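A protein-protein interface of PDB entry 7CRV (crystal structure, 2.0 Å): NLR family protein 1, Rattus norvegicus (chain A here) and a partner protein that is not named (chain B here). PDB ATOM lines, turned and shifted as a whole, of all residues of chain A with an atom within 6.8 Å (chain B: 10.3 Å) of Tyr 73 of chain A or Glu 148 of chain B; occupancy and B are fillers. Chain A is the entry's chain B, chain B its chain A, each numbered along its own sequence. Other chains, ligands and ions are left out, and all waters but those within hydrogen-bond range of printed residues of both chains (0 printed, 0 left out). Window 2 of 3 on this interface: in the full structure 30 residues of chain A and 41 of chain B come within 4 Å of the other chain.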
ATOM      1  N   VAL A  13     -11.048 -18.665   3.038  1.00  0.00           N
ATOM      2  CA  VAL A  13     -12.119 -17.680   2.958  1.00  0.00           C
ATOM      3  C   VAL A  13     -13.433 -18.320   2.520  1.00  0.00           C
ATOM      4  O   VAL A  13     -14.488 -18.070   3.114  1.00  0.00           O
ATOM      5  CB  VAL A  13     -11.719 -16.538   1.995  1.00  0.00           C
ATOM      6  CG1 VAL A  13     -12.763 -15.415   2.031  1.00  0.00           C
ATOM      7  CG2 VAL A  13     -10.269 -16.095   2.196  1.00  0.00           C
ATOM      8  N   HIS A  15     -16.923 -19.045   0.521  1.00  0.00           N
ATOM      9  CA  HIS A  15     -18.014 -18.286  -0.080  1.00  0.00           C
ATOM     10  C   HIS A  15     -18.360 -17.021   0.689  1.00  0.00           C
ATOM     11  O   HIS A  15     -19.116 -16.188   0.177  1.00  0.00           O
ATOM     12  CB  HIS A  15     -19.277 -19.141  -0.199  1.00  0.00           C
ATOM     13  CG  HIS A  15     -19.336 -19.995  -1.429  1.00  0.00           C
ATOM     14  ND1 HIS A  15     -19.695 -19.497  -2.664  1.00  0.00           N
ATOM     15  CD2 HIS A  15     -19.152 -21.325  -1.604  1.00  0.00           C
ATOM     16  CE1 HIS A  15     -19.684 -20.473  -3.556  1.00  0.00           C
ATOM     17  NE2 HIS A  15     -19.360 -21.594  -2.936  1.00  0.00           N
ATOM     18  N   PHE A  16     -17.829 -16.850   1.891  1.00  0.00           N
ATOM     19  CA  PHE A  16     -18.342 -15.841   2.813  1.00  0.00           C
ATOM     20  C   PHE A  16     -17.389 -14.639   2.802  1.00  0.00           C
ATOM     21  O   PHE A  16     -16.631 -14.399   3.738  1.00  0.00           O
ATOM     22  CB  PHE A  16     -18.551 -16.477   4.199  1.00  0.00           C
ATOM     23  CG  PHE A  16     -19.447 -17.719   4.176  1.00  0.00           C
ATOM     24  CD1 PHE A  16     -20.767 -17.638   3.721  1.00  0.00           C
ATOM     25  CD2 PHE A  16     -18.965 -18.964   4.576  1.00  0.00           C
ATOM     26  CE1 PHE A  16     -21.606 -18.766   3.682  1.00  0.00           C
ATOM     27  CE2 PHE A  16     -19.803 -20.114   4.538  1.00  0.00           C
ATOM     28  CZ  PHE A  16     -21.122 -20.007   4.092  1.00  0.00           C
ATOM     29  N   ILE A  17     -17.457 -13.873   1.704  1.00  0.00           N
ATOM     30  CA  ILE A  17     -16.583 -12.735   1.376  1.00  0.00           C
ATOM     31  C   ILE A  17     -17.359 -11.420   1.504  1.00  0.00           C
ATOM     32  O   ILE A  17     -18.596 -11.449   1.561  1.00  0.00           O
ATOM     33  CB  ILE A  17     -16.022 -12.870  -0.051  1.00  0.00           C
ATOM     34  CG1 ILE A  17     -17.159 -12.766  -1.071  1.00  0.00           C
ATOM     35  CG2 ILE A  17     -15.252 -14.186  -0.234  1.00  0.00           C
ATOM     36  CD1 ILE A  17     -16.707 -12.288  -2.442  1.00  0.00           C
ATOM     37  N   PRO A  18     -16.687 -10.232   1.523  1.00  0.00           N
ATOM     38  CA  PRO A  18     -17.428  -8.958   1.639  1.00  0.00           C
ATOM     39  C   PRO A  18     -17.938  -8.439   0.304  1.00  0.00           C
ATOM     40  O   PRO A  18     -17.158  -8.347  -0.655  1.00  0.00           O
ATOM     41  CB  PRO A  18     -16.381  -8.007   2.219  1.00  0.00           C
ATOM     42  CG  PRO A  18     -15.087  -8.494   1.610  1.00  0.00           C
ATOM     43  CD  PRO A  18     -15.236  -9.990   1.408  1.00  0.00           C
ATOM     44  N   ILE A  19     -19.229  -8.064   0.227  1.00  0.00           N
ATOM     45  CA  ILE A  19     -19.874  -7.678  -1.025  1.00  0.00           C
ATOM     46  C   ILE A  19     -20.714  -6.409  -0.859  1.00  0.00           C
ATOM     47  O   ILE A  19     -21.161  -6.057   0.232  1.00  0.00           O
ATOM     48  CB  ILE A  19     -20.784  -8.803  -1.588  1.00  0.00           C
ATOM     49  CG1 ILE A  19     -21.973  -9.032  -0.673  1.00  0.00           C
ATOM     50  CG2 ILE A  19     -20.020 -10.119  -1.806  1.00  0.00           C
ATOM     51  CD1 ILE A  19     -22.996  -9.918  -1.292  1.00  0.00           C
ATOM     52  N   ALA A  71     -19.944  -2.467   3.064  1.00  0.00           N
ATOM     53  CA  ALA A  71     -19.871  -3.835   2.552  1.00  0.00           C
ATOM     54  C   ALA A  71     -20.294  -4.836   3.625  1.00  0.00           C
ATOM     55  O   ALA A  71     -19.980  -4.681   4.808  1.00  0.00           O
ATOM     56  CB  ALA A  71     -18.456  -4.148   2.070  1.00  0.00           C
ATOM     57  N   LEU A  72     -21.059  -5.846   3.213  1.00  0.00           N
ATOM     58  CA  LEU A  72     -21.513  -6.910   4.095  1.00  0.00           C
ATOM     59  C   LEU A  72     -20.928  -8.231   3.610  1.00  0.00           C
ATOM     60  O   LEU A  72     -20.601  -8.390   2.425  1.00  0.00           O
ATOM     61  CB  LEU A  72     -23.048  -6.996   4.145  1.00  0.00           C
ATOM     62  CG  LEU A  72     -23.810  -5.678   4.405  1.00  0.00           C
ATOM     63  CD1 LEU A  72     -25.319  -5.868   4.339  1.00  0.00           C
ATOM     64  CD2 LEU A  72     -23.406  -5.060   5.748  1.00  0.00           C
ATOM     65  N   TYR A  73     -20.804  -9.174   4.544  1.00  0.00           N
ATOM     66  CA  TYR A  73     -20.160 -10.452   4.280  1.00  0.00           C
ATOM     67  C   TYR A  73     -21.219 -11.472   3.886  1.00  0.00           C
ATOM     68  O   TYR A  73     -22.290 -11.527   4.489  1.00  0.00           O
ATOM     69  CB  TYR A  73     -19.360 -10.918   5.507  1.00  0.00           C
ATOM     70  CG  TYR A  73     -17.981 -10.294   5.532  1.00  0.00           C
ATOM     71  CD1 TYR A  73     -17.770  -9.053   6.120  1.00  0.00           C
ATOM     72  CD2 TYR A  73     -16.898 -10.919   4.920  1.00  0.00           C
ATOM     73  CE1 TYR A  73     -16.509  -8.450   6.109  1.00  0.00           C
ATOM     74  CE2 TYR A  73     -15.630 -10.328   4.907  1.00  0.00           C
ATOM     75  CZ  TYR A  73     -15.437  -9.092   5.506  1.00  0.00           C
ATOM     76  OH  TYR A  73     -14.181  -8.493   5.496  1.00  0.00           O
ATOM     77  N   VAL A  74     -20.940 -12.239   2.829  1.00  0.00           N
ATOM     78  CA  VAL A  74     -21.854 -13.308   2.459  1.00  0.00           C
ATOM     79  C   VAL A  74     -22.028 -14.239   3.648  1.00  0.00           C
ATOM     80  O   VAL A  74     -21.072 -14.543   4.365  1.00  0.00           O
ATOM     81  CB  VAL A  74     -21.342 -14.056   1.216  1.00  0.00           C
ATOM     82  CG1 VAL A  74     -22.131 -15.340   0.983  1.00  0.00           C
ATOM     83  CG2 VAL A  74     -21.451 -13.146   0.008  1.00  0.00           C
ATOM     84  N   GLY A  75     -23.259 -14.655   3.888  1.00  0.00           N
ATOM     85  CA  GLY A  75     -23.565 -15.505   5.010  1.00  0.00           C
ATOM     86  C   GLY A  75     -23.833 -14.786   6.309  1.00  0.00           C
ATOM     87  O   GLY A  75     -24.350 -15.414   7.240  1.00  0.00           O
ATOM     88  N   SER A  76     -23.500 -13.497   6.427  1.00  0.00           N
ATOM     89  CA  SER A  76     -23.842 -12.797   7.662  1.00  0.00           C
ATOM     90  C   SER A  76     -25.359 -12.715   7.789  1.00  0.00           C
ATOM     91  O   SER A  76     -26.098 -12.814   6.802  1.00  0.00           O
ATOM     92  CB  SER A  76     -23.174 -11.407   7.728  1.00  0.00           C
ATOM     93  OG  SER A  76     -23.349 -10.629   6.549  1.00  0.00           O
ATOM     94  N   ARG A  77     -25.827 -12.620   9.037  1.00  0.00           N
ATOM     95  CA  ARG A  77     -27.244 -12.644   9.372  1.00  0.00           C
ATOM     96  C   ARG A  77     -27.657 -11.334  10.027  1.00  0.00           C
ATOM     97  O   ARG A  77     -26.882 -10.714  10.762  1.00  0.00           O
ATOM     98  CB  ARG A  77     -27.560 -13.820  10.288  1.00  0.00           C
ATOM     99  CG  ARG A  77     -27.012 -15.092   9.678  1.00  0.00           C
ATOM    100  CD  ARG A  77     -27.883 -16.318   9.887  1.00  0.00           C
ATOM    101  NE  ARG A  77     -27.411 -17.362   8.976  1.00  0.00           N
ATOM    102  CZ  ARG A  77     -26.798 -18.481   9.348  1.00  0.00           C
ATOM    103  NH1 ARG A  77     -26.587 -18.746  10.634  1.00  0.00           N
ATOM    104  NH2 ARG A  77     -26.402 -19.347   8.425  1.00  0.00           N
ATOM    105  N   TYR A  78     -28.888 -10.915   9.730  1.00  0.00           N
ATOM    106  CA  TYR A  78     -29.408  -9.610  10.121  1.00  0.00           C
ATOM    107  C   TYR A  78     -30.794  -9.804  10.689  1.00  0.00           C
ATOM    108  O   TYR A  78     -31.522 -10.685  10.240  1.00  0.00           O
ATOM    109  CB  TYR A  78     -29.422  -8.636   8.908  1.00  0.00           C
ATOM    110  CG  TYR A  78     -28.013  -8.475   8.398  1.00  0.00           C
ATOM    111  CD1 TYR A  78     -27.126  -7.615   9.033  1.00  0.00           C
ATOM    112  CD2 TYR A  78     -27.528  -9.277   7.366  1.00  0.00           C
ATOM    113  CE1 TYR A  78     -25.818  -7.517   8.626  1.00  0.00           C
ATOM    114  CE2 TYR A  78     -26.219  -9.176   6.946  1.00  0.00           C
ATOM    115  CZ  TYR A  78     -25.373  -8.286   7.586  1.00  0.00           C
ATOM    116  OH  TYR A  78     -24.074  -8.181   7.192  1.00  0.00           O
ATOM    117  N   LEU A  95     -27.630 -12.956   4.173  1.00  0.00           N
ATOM    118  CA  LEU A  95     -27.133 -12.431   2.909  1.00  0.00           C
ATOM    119  C   LEU A  95     -26.446 -13.566   2.151  1.00  0.00           C
ATOM    120  O   LEU A  95     -25.385 -14.049   2.560  1.00  0.00           O
ATOM    121  CB  LEU A  95     -26.182 -11.263   3.139  1.00  0.00           C
ATOM    122  CG  LEU A  95     -25.554 -10.682   1.874  1.00  0.00           C
ATOM    123  CD1 LEU A  95     -26.624 -10.217   0.886  1.00  0.00           C
ATOM    124  CD2 LEU A  95     -24.633  -9.538   2.207  1.00  0.00           C
ATOM    125  N   CYS A  96     -27.039 -13.989   1.039  1.00  0.00           N
ATOM    126  CA  CYS A  96     -26.395 -15.003   0.212  1.00  0.00           C
ATOM    127  C   CYS A  96     -26.761 -14.775  -1.248  1.00  0.00           C
ATOM    128  O   CYS A  96     -27.731 -14.085  -1.571  1.00  0.00           O
ATOM    129  CB  CYS A  96     -26.808 -16.412   0.636  1.00  0.00           C
ATOM    130  SG  CYS A  96     -28.583 -16.527   0.786  1.00  0.00           S
ATOM    131  N   MET B 120     -16.369 -18.527  -7.647  1.00  0.00           N
ATOM    132  CA  MET B 120     -17.625 -18.032  -7.114  1.00  0.00           C
ATOM    133  C   MET B 120     -18.231 -17.031  -8.084  1.00  0.00           C
ATOM    134  O   MET B 120     -17.505 -16.220  -8.673  1.00  0.00           O
ATOM    135  CB  MET B 120     -17.363 -17.320  -5.800  1.00  0.00           C
ATOM    136  CG  MET B 120     -17.451 -18.133  -4.564  1.00  0.00           C
ATOM    137  SD  MET B 120     -16.478 -17.193  -3.410  1.00  0.00           S
ATOM    138  CE  MET B 120     -17.240 -15.584  -3.663  1.00  0.00           C
ATOM    139  N   HIS B 142     -19.408  -6.229 -11.068  1.00  0.00           N
ATOM    140  CA  HIS B 142     -19.229  -7.254 -10.054  1.00  0.00           C
ATOM    141  C   HIS B 142     -19.589  -6.638  -8.716  1.00  0.00           C
ATOM    142  O   HIS B 142     -19.438  -5.428  -8.526  1.00  0.00           O
ATOM    143  CB  HIS B 142     -17.789  -7.799 -10.052  1.00  0.00           C
ATOM    144  CG  HIS B 142     -16.775  -6.845  -9.486  1.00  0.00           C
ATOM    145  ND1 HIS B 142     -16.702  -6.544  -8.143  1.00  0.00           N
ATOM    146  CD2 HIS B 142     -15.786  -6.129 -10.085  1.00  0.00           C
ATOM    147  CE1 HIS B 142     -15.713  -5.687  -7.938  1.00  0.00           C
ATOM    148  NE2 HIS B 142     -15.137  -5.429  -9.098  1.00  0.00           N
ATOM    149  N   PHE B 143     -20.070  -7.462  -7.781  1.00  0.00           N
ATOM    150  CA  PHE B 143     -20.463  -6.948  -6.474  1.00  0.00           C
ATOM    151  C   PHE B 143     -19.442  -7.234  -5.369  1.00  0.00           C
ATOM    152  O   PHE B 143     -19.773  -7.100  -4.188  1.00  0.00           O
ATOM    153  CB  PHE B 143     -21.842  -7.483  -6.075  1.00  0.00           C
ATOM    154  CG  PHE B 143     -22.027  -8.960  -6.311  1.00  0.00           C
ATOM    155  CD1 PHE B 143     -21.421  -9.899  -5.481  1.00  0.00           C
ATOM    156  CD2 PHE B 143     -22.849  -9.403  -7.329  1.00  0.00           C
ATOM    157  CE1 PHE B 143     -21.620 -11.244  -5.698  1.00  0.00           C
ATOM    158  CE2 PHE B 143     -23.060 -10.748  -7.553  1.00  0.00           C
ATOM    159  CZ  PHE B 143     -22.442 -11.676  -6.735  1.00  0.00           C
ATOM    160  N   VAL B 144     -18.214  -7.601  -5.705  1.00  0.00           N
ATOM    161  CA  VAL B 144     -17.197  -7.807  -4.667  1.00  0.00           C
ATOM    162  C   VAL B 144     -16.719  -6.448  -4.169  1.00  0.00           C
ATOM    163  O   VAL B 144     -16.480  -5.531  -4.959  1.00  0.00           O
ATOM    164  CB  VAL B 144     -16.016  -8.642  -5.204  1.00  0.00           C
ATOM    165  CG1 VAL B 144     -15.059  -9.025  -4.061  1.00  0.00           C
ATOM    166  CG2 VAL B 144     -16.521  -9.889  -5.894  1.00  0.00           C
ATOM    167  N   SER B 145     -16.566  -6.315  -2.857  1.00  0.00           N
ATOM    168  CA  SER B 145     -16.018  -5.092  -2.286  1.00  0.00           C
ATOM    169  C   SER B 145     -14.493  -5.157  -2.299  1.00  0.00           C
ATOM    170  O   SER B 145     -13.898  -6.110  -1.789  1.00  0.00           O
ATOM    171  CB  SER B 145     -16.531  -4.887  -0.861  1.00  0.00           C
ATOM    172  OG  SER B 145     -15.870  -3.774  -0.271  1.00  0.00           O
ATOM    173  N   LEU B 146     -13.864  -4.150  -2.901  1.00  0.00           N
ATOM    174  CA  LEU B 146     -12.413  -4.050  -2.950  1.00  0.00           C
ATOM    175  C   LEU B 146     -11.868  -2.938  -2.066  1.00  0.00           C
ATOM    176  O   LEU B 146     -10.643  -2.766  -1.997  1.00  0.00           O
ATOM    177  CB  LEU B 146     -11.943  -3.837  -4.395  1.00  0.00           C
ATOM    178  CG  LEU B 146     -12.401  -4.930  -5.361  1.00  0.00           C
ATOM    179  CD1 LEU B 146     -11.870  -4.707  -6.770  1.00  0.00           C
ATOM    180  CD2 LEU B 146     -11.969  -6.277  -4.820  1.00  0.00           C
ATOM    181  N   GLN B 147     -12.736  -2.175  -1.396  1.00  0.00           N
ATOM    182  CA  GLN B 147     -12.266  -1.035  -0.612  1.00  0.00           C
ATOM    183  C   GLN B 147     -11.345  -1.485   0.508  1.00  0.00           C
ATOM    184  O   GLN B 147     -10.364  -0.800   0.829  1.00  0.00           O
ATOM    185  CB  GLN B 147     -13.450  -0.247  -0.052  1.00  0.00           C
ATOM    186  CG  GLN B 147     -14.595  -0.116  -1.034  1.00  0.00           C
ATOM    187  CD  GLN B 147     -14.208   0.697  -2.263  1.00  0.00           C
ATOM    188  OE1 GLN B 147     -13.372   1.605  -2.187  1.00  0.00           O
ATOM    189  NE2 GLN B 147     -14.815   0.373  -3.403  1.00  0.00           N
ATOM    190  N   GLU B 148     -11.640  -2.634   1.109  1.00  0.00           N
ATOM    191  CA  GLU B 148     -10.732  -3.247   2.064  1.00  0.00           C
ATOM    192  C   GLU B 148      -9.718  -4.099   1.315  1.00  0.00           C
ATOM    193  O   GLU B 148     -10.062  -4.780   0.342  1.00  0.00           O
ATOM    194  CB  GLU B 148     -11.500  -4.097   3.077  1.00  0.00           C
ATOM    195  CG  GLU B 148     -10.708  -4.374   4.357  1.00  0.00           C
ATOM    196  CD  GLU B 148     -11.557  -4.972   5.488  1.00  0.00           C
ATOM    197  OE1 GLU B 148     -12.726  -5.358   5.248  1.00  0.00           O
ATOM    198  OE2 GLU B 148     -11.050  -5.039   6.631  1.00  0.00           O
ATOM    199  N   GLY B 149      -8.467  -4.051   1.768  1.00  0.00           N
ATOM    200  CA  GLY B 149      -7.412  -4.851   1.174  1.00  0.00           C
ATOM    201  C   GLY B 149      -7.544  -6.323   1.512  1.00  0.00           C
ATOM    202  O   GLY B 149      -6.627  -6.918   2.085  1.00  0.00           O
ATOM    203  N   LYS B 150      -8.695  -6.915   1.172  1.00  0.00           N
ATOM    204  CA  LYS B 150      -8.977  -8.315   1.448  1.00  0.00           C
ATOM    205  C   LYS B 150      -9.078  -9.185   0.207  1.00  0.00           C
ATOM    206  O   LYS B 150      -8.994 -10.413   0.330  1.00  0.00           O
ATOM    207  CB  LYS B 150     -10.284  -8.465   2.244  1.00  0.00           C
ATOM    208  CG  LYS B 150     -10.263  -7.844   3.634  1.00  0.00           C
ATOM    209  CD  LYS B 150      -9.031  -8.295   4.411  1.00  0.00           C
ATOM    210  CE  LYS B 150      -9.050  -9.805   4.693  1.00  0.00           C
ATOM    211  NZ  LYS B 150      -7.810 -10.271   5.377  1.00  0.00           N
ATOM    212  N   VAL B 151      -9.260  -8.599  -0.973  1.00  0.00           N
ATOM    213  CA  VAL B 151      -9.495  -9.376  -2.185  1.00  0.00           C
ATOM    214  C   VAL B 151      -8.372  -9.104  -3.183  1.00  0.00           C
ATOM    215  O   VAL B 151      -8.189  -7.967  -3.631  1.00  0.00           O
ATOM    216  CB  VAL B 151     -10.875  -9.073  -2.792  1.00  0.00           C
ATOM    217  CG1 VAL B 151     -11.104  -9.955  -4.005  1.00  0.00           C
ATOM    218  CG2 VAL B 151     -11.982  -9.293  -1.740  1.00  0.00           C
ATOM    219  N   ASP B 152      -7.641 -10.156  -3.543  1.00  0.00           N
ATOM    220  CA  ASP B 152      -6.590 -10.082  -4.549  1.00  0.00           C
ATOM    221  C   ASP B 152      -7.204  -9.873  -5.932  1.00  0.00           C
ATOM    222  O   ASP B 152      -8.020 -10.681  -6.381  1.00  0.00           O
ATOM    223  CB  ASP B 152      -5.781 -11.372  -4.507  1.00  0.00           C
ATOM    224  CG  ASP B 152      -4.592 -11.376  -5.448  1.00  0.00           C
ATOM    225  OD1 ASP B 152      -3.728 -12.246  -5.190  1.00  0.00           O
ATOM    226  OD2 ASP B 152      -4.500 -10.576  -6.410  1.00  0.00           O
ATOM    227  N   SER B 153      -6.772  -8.825  -6.645  1.00  0.00           N
ATOM    228  CA  SER B 153      -7.377  -8.538  -7.949  1.00  0.00           C
ATOM    229  C   SER B 153      -7.025  -9.560  -9.022  1.00  0.00           C
ATOM    230  O   SER B 153      -7.806  -9.737  -9.969  1.00  0.00           O
ATOM    231  CB  SER B 153      -6.989  -7.138  -8.411  1.00  0.00           C
ATOM    232  OG  SER B 153      -7.756  -6.195  -7.680  1.00  0.00           O
ATOM    233  N   PHE B 156      -9.797 -12.435 -10.049  1.00  0.00           N
ATOM    234  CA  PHE B 156     -10.981 -12.178 -10.868  1.00  0.00           C
ATOM    235  C   PHE B 156     -10.798 -12.754 -12.269  1.00  0.00           C
ATOM    236  O   PHE B 156      -9.723 -12.655 -12.861  1.00  0.00           O
ATOM    237  CB  PHE B 156     -11.239 -10.669 -10.972  1.00  0.00           C
ATOM    238  CG  PHE B 156     -11.802 -10.040  -9.715  1.00  0.00           C
ATOM    239  CD1 PHE B 156     -13.174  -9.906  -9.547  1.00  0.00           C
ATOM    240  CD2 PHE B 156     -10.965  -9.543  -8.727  1.00  0.00           C
ATOM    241  CE1 PHE B 156     -13.697  -9.300  -8.401  1.00  0.00           C
ATOM    242  CE2 PHE B 156     -11.477  -8.957  -7.577  1.00  0.00           C
ATOM    243  CZ  PHE B 156     -12.840  -8.836  -7.414  1.00  0.00           C
ATOM    244  N   PRO B 176     -13.266  -0.961  -8.800  1.00  0.00           N
ATOM    245  CA  PRO B 176     -14.081  -1.238  -7.605  1.00  0.00           C
ATOM    246  C   PRO B 176     -15.380  -1.975  -7.874  1.00  0.00           C
ATOM    247  O   PRO B 176     -15.794  -2.783  -7.034  1.00  0.00           O
ATOM    248  CB  PRO B 176     -14.351   0.169  -7.043  1.00  0.00           C
ATOM    249  CG  PRO B 176     -13.162   0.960  -7.443  1.00  0.00           C
ATOM    250  CD  PRO B 176     -12.763   0.430  -8.799  1.00  0.00           C
ATOM    251  N   HIS B 177     -16.048  -1.722  -9.008  1.00  0.00           N
ATOM    252  CA  HIS B 177     -17.377  -2.280  -9.238  1.00  0.00           C
ATOM    253  C   HIS B 177     -17.536  -2.914 -10.615  1.00  0.00           C
ATOM    254  O   HIS B 177     -18.660  -3.297 -10.983  1.00  0.00           O
ATOM    255  CB  HIS B 177     -18.458  -1.209  -9.033  1.00  0.00           C
ATOM    256  CG  HIS B 177     -18.459  -0.621  -7.660  1.00  0.00           C
ATOM    257  ND1 HIS B 177     -17.984   0.647  -7.391  1.00  0.00           N
ATOM    258  CD2 HIS B 177     -18.863  -1.131  -6.470  1.00  0.00           C
ATOM    259  CE1 HIS B 177     -18.101   0.895  -6.098  1.00  0.00           C
ATOM    260  NE2 HIS B 177     -18.631  -0.167  -5.516  1.00  0.00           N
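The side-chain hydroxyl (OH) of Tyr 73 of chain A lies within hydrogen-bond range of the side-chain carboxylate (OE1) of Glu 148 of chain B, at 3.5 Å.
The backbone NH of Ser 145 of chain B is in hydrogen-bond range of the backbone carbonyl oxygen of Pro 18 of chain A.
The backbone carbonyl oxygen (O) of Tyr 73 of chain A lies within hydrogen-bond range of the side-chain hydroxyl (OG) of Ser 76 of chain A (2.5 Å).
The backbone carbonyl oxygen (O) of Ile 17 of chain A sits at hydrogen-bond distance from the backbone NH (N) of Val 74 of chain A (2.8 Å).
The backbone NH of Ile 19 of chain A sits at hydrogen-bond distance from the backbone carbonyl oxygen of Leu 72 of chain A (2.6 Å).
A ring nitrogen (ND1) of His 142 of chain B sits at hydrogen-bond distance from the backbone NH of Val 144 of chain B, 3.1 Å away.
ND1 of His 15 of chain A touches CG of Met 120 of chain B (3.2 Å).
Ile 17 of chain A touches Met 120 of chain B (CD1 to CE, 3.6 Å).
Val 144 of chain B touches Ile 17 of chain A (CG1 to CD1, 3.998 Å).
Ile 19 of chain A touches Phe 143 of chain B (CA to O, 3.2 Å).
Ala 71 of chain A touches Ser 145 of chain B (CB to OG, 3.5 Å).
Of chain B, only Glu 148 comes within 4 Å of Tyr 73 of chain A.
Glu 148 of chain B touches just one residue of chain A: Tyr 73.
No residue of chain B comes within 4 Å of Leu 72 of chain A.
Ser 76 of chain A touches none of the printed residues of chain B.
Leu 95 of chain A touches none of the printed residues of chain B.
Of the printed residues of chain A, Ser 145 of chain B touches Pro 18 (3.1 Å) and Ala 71 (3.5 Å).
Of the printed residues of chain A, Phe 143 of chain B touches Ile 19.
Of the printed residues of chain B, Ile 19 of chain A touches Phe 143 (3.2 Å).
Printed residues of chain B within 4 Å of His 15 of chain A: Met 120 (3.2 Å).
Of the printed residues of chain A, Met 120 of chain B touches His 15 (3.2 Å) and Ile 17 (3.6 Å).
Asp 152 of chain B touches none of the printed residues of chain A.
Val 151 of chain B touches none of the printed residues of chain A.
Of the 16 printed residues of chain A, 6 touch a printed residue of chain B.
Hydrophobic or aromatic side chains of chain A that line the printed part of chain B: His 15, Ile 17, Ile 19, Ala 71 and Tyr 73.
Of the 16 printed residues of chain B, 5 touch a printed residue of chain A.
Among the printed residues, 7 pairs touch across the chains.
Among the printed residues, no Asp or Glu carboxylate lies within 4 Å of a Lys or Arg side-chain nitrogen of the other chain.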
